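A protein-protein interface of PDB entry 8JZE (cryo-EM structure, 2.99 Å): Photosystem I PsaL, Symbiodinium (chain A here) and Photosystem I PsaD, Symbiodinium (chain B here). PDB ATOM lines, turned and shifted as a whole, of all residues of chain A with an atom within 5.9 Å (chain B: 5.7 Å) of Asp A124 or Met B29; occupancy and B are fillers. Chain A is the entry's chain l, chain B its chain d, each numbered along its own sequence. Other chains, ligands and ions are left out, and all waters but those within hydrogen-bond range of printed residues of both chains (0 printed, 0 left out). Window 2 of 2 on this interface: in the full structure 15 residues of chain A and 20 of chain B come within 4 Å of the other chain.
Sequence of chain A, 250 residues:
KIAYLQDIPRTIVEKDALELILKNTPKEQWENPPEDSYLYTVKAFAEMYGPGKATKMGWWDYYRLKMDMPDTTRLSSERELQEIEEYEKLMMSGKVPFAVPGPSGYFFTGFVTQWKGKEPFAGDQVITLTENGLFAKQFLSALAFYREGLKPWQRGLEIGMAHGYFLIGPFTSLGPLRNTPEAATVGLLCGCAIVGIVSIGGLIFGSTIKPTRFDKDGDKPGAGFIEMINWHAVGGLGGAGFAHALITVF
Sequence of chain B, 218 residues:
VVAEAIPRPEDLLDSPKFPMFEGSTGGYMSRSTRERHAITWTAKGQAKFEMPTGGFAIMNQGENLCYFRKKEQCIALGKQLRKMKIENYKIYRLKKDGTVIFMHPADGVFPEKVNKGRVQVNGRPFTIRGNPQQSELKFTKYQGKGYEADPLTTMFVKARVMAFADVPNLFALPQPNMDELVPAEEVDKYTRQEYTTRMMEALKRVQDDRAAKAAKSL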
ATOM      1  N   ALA A 122      21.382   0.554   9.326  1.00  0.00           N
ATOM      2  CA  ALA A 122      22.345   1.177   8.427  1.00  0.00           C
ATOM      3  C   ALA A 122      22.686   0.227   7.286  1.00  0.00           C
ATOM      4  O   ALA A 122      22.944  -0.959   7.510  1.00  0.00           O
ATOM      5  CB  ALA A 122      23.612   1.570   9.183  1.00  0.00           C
ATOM      6  N   GLY A 123      22.684   0.753   6.060  1.00  0.00           N
ATOM      7  CA  GLY A 123      22.935  -0.086   4.903  1.00  0.00           C
ATOM      8  C   GLY A 123      24.394  -0.398   4.662  1.00  0.00           C
ATOM      9  O   GLY A 123      24.716  -1.449   4.100  1.00  0.00           O
ATOM     10  N   ASP A 124      25.292   0.494   5.068  1.00  0.00           N
ATOM     11  CA  ASP A 124      26.716   0.316   4.827  1.00  0.00           C
ATOM     12  C   ASP A 124      27.446  -0.322   5.999  1.00  0.00           C
ATOM     13  O   ASP A 124      28.665  -0.506   5.924  1.00  0.00           O
ATOM     14  CB  ASP A 124      27.373   1.658   4.495  1.00  0.00           C
ATOM     15  CG  ASP A 124      27.317   2.638   5.648  1.00  0.00           C
ATOM     16  OD1 ASP A 124      26.391   2.533   6.480  1.00  0.00           O
ATOM     17  OD2 ASP A 124      28.198   3.519   5.723  1.00  0.00           O
ATOM     18  N   GLN A 125      26.745  -0.652   7.078  1.00  0.00           N
ATOM     19  CA  GLN A 125      27.371  -1.297   8.220  1.00  0.00           C
ATOM     20  C   GLN A 125      27.173  -2.805   8.229  1.00  0.00           C
ATOM     21  O   GLN A 125      27.622  -3.466   9.170  1.00  0.00           O
ATOM     22  CB  GLN A 125      26.849  -0.691   9.527  1.00  0.00           C
ATOM     23  CG  GLN A 125      27.121   0.802   9.655  1.00  0.00           C
ATOM     24  CD  GLN A 125      27.233   1.259  11.096  1.00  0.00           C
ATOM     25  OE1 GLN A 125      27.525   0.468  11.991  1.00  0.00           O
ATOM     26  NE2 GLN A 125      27.003   2.546  11.327  1.00  0.00           N
ATOM     27  N   VAL A 126      26.522  -3.366   7.208  1.00  0.00           N
ATOM     28  CA  VAL A 126      26.427  -4.817   7.101  1.00  0.00           C
ATOM     29  C   VAL A 126      27.834  -5.377   6.946  1.00  0.00           C
ATOM     30  O   VAL A 126      28.513  -5.134   5.941  1.00  0.00           O
ATOM     31  CB  VAL A 126      25.513  -5.222   5.939  1.00  0.00           C
ATOM     32  CG1 VAL A 126      24.059  -5.027   6.325  1.00  0.00           C
ATOM     33  CG2 VAL A 126      25.827  -4.412   4.693  1.00  0.00           C
ATOM     34  N   GLU A 131      35.750  -6.450   4.336  1.00  0.00           N
ATOM     35  CA  GLU A 131      35.849  -5.080   4.823  1.00  0.00           C
ATOM     36  C   GLU A 131      35.824  -5.025   6.345  1.00  0.00           C
ATOM     37  O   GLU A 131      36.395  -4.109   6.946  1.00  0.00           O
ATOM     38  CB  GLU A 131      34.721  -4.219   4.252  1.00  0.00           C
ATOM     39  CG  GLU A 131      34.903  -2.724   4.491  1.00  0.00           C
ATOM     40  CD  GLU A 131      33.672  -1.916   4.136  1.00  0.00           C
ATOM     41  OE1 GLU A 131      32.637  -2.529   3.807  1.00  0.00           O
ATOM     42  OE2 GLU A 131      33.739  -0.669   4.188  1.00  0.00           O
ATOM     43  N   ASN A 132      35.169  -5.996   6.978  1.00  0.00           N
ATOM     44  CA  ASN A 132      35.015  -5.992   8.424  1.00  0.00           C
ATOM     45  C   ASN A 132      35.698  -7.163   9.110  1.00  0.00           C
ATOM     46  O   ASN A 132      35.585  -7.293  10.334  1.00  0.00           O
ATOM     47  CB  ASN A 132      33.527  -5.969   8.793  1.00  0.00           C
ATOM     48  CG  ASN A 132      32.806  -4.773   8.209  1.00  0.00           C
ATOM     49  OD1 ASN A 132      32.366  -4.800   7.062  1.00  0.00           O
ATOM     50  ND2 ASN A 132      32.685  -3.711   8.997  1.00  0.00           N
ATOM     51  N   SER B  24      19.702  -5.473   5.181  1.00  0.00           N
ATOM     52  CA  SER B  24      20.221  -5.494   3.824  1.00  0.00           C
ATOM     53  C   SER B  24      21.095  -4.267   3.605  1.00  0.00           C
ATOM     54  O   SER B  24      21.288  -3.444   4.505  1.00  0.00           O
ATOM     55  CB  SER B  24      19.079  -5.547   2.802  1.00  0.00           C
ATOM     56  OG  SER B  24      18.269  -4.389   2.883  1.00  0.00           O
ATOM     57  N   THR B  25      21.633  -4.149   2.390  1.00  0.00           N
ATOM     58  CA  THR B  25      22.403  -2.971   2.014  1.00  0.00           C
ATOM     59  C   THR B  25      21.522  -1.770   1.708  1.00  0.00           C
ATOM     60  O   THR B  25      22.049  -0.667   1.524  1.00  0.00           O
ATOM     61  CB  THR B  25      23.283  -3.272   0.797  1.00  0.00           C
ATOM     62  OG1 THR B  25      22.455  -3.550  -0.338  1.00  0.00           O
ATOM     63  CG2 THR B  25      24.178  -4.466   1.070  1.00  0.00           C
ATOM     64  N   GLY B  27      19.560  -0.170   3.670  1.00  0.00           N
ATOM     65  CA  GLY B  27      19.369   0.731   4.786  1.00  0.00           C
ATOM     66  C   GLY B  27      20.075   2.056   4.576  1.00  0.00           C
ATOM     67  O   GLY B  27      20.847   2.248   3.636  1.00  0.00           O
ATOM     68  N   TYR B  28      19.793   2.993   5.480  1.00  0.00           N
ATOM     69  CA  TYR B  28      20.331   4.340   5.346  1.00  0.00           C
ATOM     70  C   TYR B  28      21.853   4.313   5.352  1.00  0.00           C
ATOM     71  O   TYR B  28      22.480   3.581   6.123  1.00  0.00           O
ATOM     72  CB  TYR B  28      19.804   5.246   6.463  1.00  0.00           C
ATOM     73  CG  TYR B  28      20.243   4.877   7.862  1.00  0.00           C
ATOM     74  CD1 TYR B  28      21.424   5.373   8.396  1.00  0.00           C
ATOM     75  CD2 TYR B  28      19.462   4.055   8.660  1.00  0.00           C
ATOM     76  CE1 TYR B  28      21.824   5.045   9.673  1.00  0.00           C
ATOM     77  CE2 TYR B  28      19.853   3.726   9.942  1.00  0.00           C
ATOM     78  CZ  TYR B  28      21.035   4.224  10.442  1.00  0.00           C
ATOM     79  OH  TYR B  28      21.430   3.898  11.717  1.00  0.00           O
ATOM     80  N   MET B  29      22.447   5.118   4.477  1.00  0.00           N
ATOM     81  CA  MET B  29      23.892   5.122   4.277  1.00  0.00           C
ATOM     82  C   MET B  29      24.536   5.979   5.355  1.00  0.00           C
ATOM     83  O   MET B  29      24.567   7.208   5.254  1.00  0.00           O
ATOM     84  CB  MET B  29      24.232   5.637   2.882  1.00  0.00           C
ATOM     85  CG  MET B  29      25.686   5.464   2.467  1.00  0.00           C
ATOM     86  SD  MET B  29      26.118   3.755   2.096  1.00  0.00           S
ATOM     87  CE  MET B  29      24.570   3.148   1.436  1.00  0.00           C
ATOM     88  N   SER B  30      25.057   5.336   6.396  1.00  0.00           N
ATOM     89  CA  SER B  30      25.837   6.057   7.388  1.00  0.00           C
ATOM     90  C   SER B  30      27.158   6.510   6.768  1.00  0.00           C
ATOM     91  O   SER B  30      27.465   6.220   5.608  1.00  0.00           O
ATOM     92  CB  SER B  30      26.066   5.191   8.624  1.00  0.00           C
ATOM     93  OG  SER B  30      26.738   3.990   8.296  1.00  0.00           O
ATOM     94  N   ARG B  31      27.929   7.272   7.547  1.00  0.00           N
ATOM     95  CA  ARG B  31      29.228   7.809   7.144  1.00  0.00           C
ATOM     96  C   ARG B  31      29.082   8.868   6.056  1.00  0.00           C
ATOM     97  O   ARG B  31      30.068   9.495   5.657  1.00  0.00           O
ATOM     98  CB  ARG B  31      30.166   6.689   6.675  1.00  0.00           C
ATOM     99  CG  ARG B  31      30.315   5.546   7.667  1.00  0.00           C
ATOM    100  CD  ARG B  31      31.091   4.378   7.077  1.00  0.00           C
ATOM    101  NE  ARG B  31      31.066   3.211   7.953  1.00  0.00           N
ATOM    102  CZ  ARG B  31      31.631   2.046   7.668  1.00  0.00           C
ATOM    103  NH1 ARG B  31      32.283   1.854   6.532  1.00  0.00           N
ATOM    104  NH2 ARG B  31      31.541   1.049   8.543  1.00  0.00           N
ATOM    105  N   SER B  32      27.858   9.075   5.570  1.00  0.00           N
ATOM    106  CA  SER B  32      27.574  10.146   4.618  1.00  0.00           C
ATOM    107  C   SER B  32      26.298  10.919   4.911  1.00  0.00           C
ATOM    108  O   SER B  32      26.193  12.070   4.478  1.00  0.00           O
ATOM    109  CB  SER B  32      27.491   9.590   3.193  1.00  0.00           C
ATOM    110  OG  SER B  32      26.407   8.691   3.064  1.00  0.00           O
ATOM    111  N   THR B  33      25.327  10.347   5.619  1.00  0.00           N
ATOM    112  CA  THR B  33      24.060  11.002   5.903  1.00  0.00           C
ATOM    113  C   THR B  33      23.837  11.052   7.407  1.00  0.00           C
ATOM    114  O   THR B  33      24.115  10.082   8.118  1.00  0.00           O
ATOM    115  CB  THR B  33      22.888  10.276   5.231  1.00  0.00           C
ATOM    116  OG1 THR B  33      22.718   8.984   5.825  1.00  0.00           O
ATOM    117  CG2 THR B  33      23.141  10.109   3.745  1.00  0.00           C
ATOM    118  N   ARG B  36      17.935  11.283   9.614  1.00  0.00           N
ATOM    119  CA  ARG B  36      17.241  10.006   9.616  1.00  0.00           C
ATOM    120  C   ARG B  36      15.782  10.222   9.982  1.00  0.00           C
ATOM    121  O   ARG B  36      15.444  11.117  10.760  1.00  0.00           O
ATOM    122  CB  ARG B  36      17.883   9.009  10.601  1.00  0.00           C
ATOM    123  CG  ARG B  36      19.125   8.290  10.076  1.00  0.00           C
ATOM    124  CD  ARG B  36      20.298   9.240   9.919  1.00  0.00           C
ATOM    125  NE  ARG B  36      21.460   8.610   9.307  1.00  0.00           N
ATOM    126  CZ  ARG B  36      22.539   8.228   9.976  1.00  0.00           C
ATOM    127  NH1 ARG B  36      22.627   8.377  11.288  1.00  0.00           N
ATOM    128  NH2 ARG B  36      23.556   7.688   9.312  1.00  0.00           N
ATOM    129  N   ARG B  69      16.265   6.564   5.988  1.00  0.00           N
ATOM    130  CA  ARG B  69      16.904   7.772   5.480  1.00  0.00           C
ATOM    131  C   ARG B  69      15.883   8.780   4.968  1.00  0.00           C
ATOM    132  O   ARG B  69      16.049   9.989   5.163  1.00  0.00           O
ATOM    133  CB  ARG B  69      17.893   7.406   4.371  1.00  0.00           C
ATOM    134  CG  ARG B  69      18.406   8.577   3.555  1.00  0.00           C
ATOM    135  CD  ARG B  69      19.209   9.547   4.395  1.00  0.00           C
ATOM    136  NE  ARG B  69      19.600  10.718   3.622  1.00  0.00           N
ATOM    137  CZ  ARG B  69      18.885  11.830   3.533  1.00  0.00           C
ATOM    138  NH1 ARG B  69      17.738  11.966   4.178  1.00  0.00           N
ATOM    139  NH2 ARG B  69      19.331  12.831   2.780  1.00  0.00           N
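Ala A122 touches Tyr B28. Gly A123 touches Ser B24 (CA to O, 3.8 Å). Gly A123 touches Thr B25 (O to CA, 3.5 Å). CB of Asp A124 touches SD of Met B29, 3.4 Å away. CG1 of Val A126 touches O of Ser B24, at 3.7 Å. CG2 of Val A126 touches CG2 of Thr B25, at 3.98 Å.
The backbone carbonyl oxygen of Gly B27 sits close to the backbone NH of Gly A123. N of Gly A123 lies within hydrogen-bond range of O of Tyr B28. OD2 of Asp A124 sits at hydrogen-bond distance from OG of Ser B30, 3.0 Å away. NE of Arg B31 lies within salt-bridge range of OD2 of Asp A124 (3.6 Å). The side-chain amide nitrogen (NE2) of Gln A125 lies within hydrogen-bond range of the side-chain hydroxyl (OG) of Ser B30. NH1 of Arg B31 lies within salt-bridge range of OE2 of Glu A131 (3.7 Å).
Of the 11 printed residues of chain B, 7 touch a printed residue of chain A. Of the 7 printed residues of chain A, 6 touch a printed residue of chain B. Hydrophobic or aromatic side chains of chain A within 4 Å of the printed part of chain B: Ala A122 and Val A126. Among the printed residues, 12 pairs touch across the chains. Among the printed residues, Asp or Glu carboxylates within 4 Å of a Lys or Arg side-chain nitrogen of the other chain: Asp A124 with Arg B31 and Glu A131 with Arg B31.
Of the printed residues of chain B, Asp A124 touches Met B29, Ser B30 and Arg B31. Of chain A, only Asp A124 (3.4 Å) comes within 4 Å of Met B29. Printed residues of chain A within 4 Å of Ser B30: Asp A124 (2.4 Å) and Gln A125 (3.4 Å). Printed residues of chain A within 4 Å of Thr B25: Gly A123 and Val A126. The nearest residue of chain B that does not touch Asp A124 is Tyr B28 (4.1 Å).
OG of Ser B32 is in hydrogen-bond range of O of Met B29, at 3.2 Å. The side-chain hydroxyl of Thr B33 lies within hydrogen-bond range of the backbone carbonyl oxygen of Met B29, at 2.6 Å.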
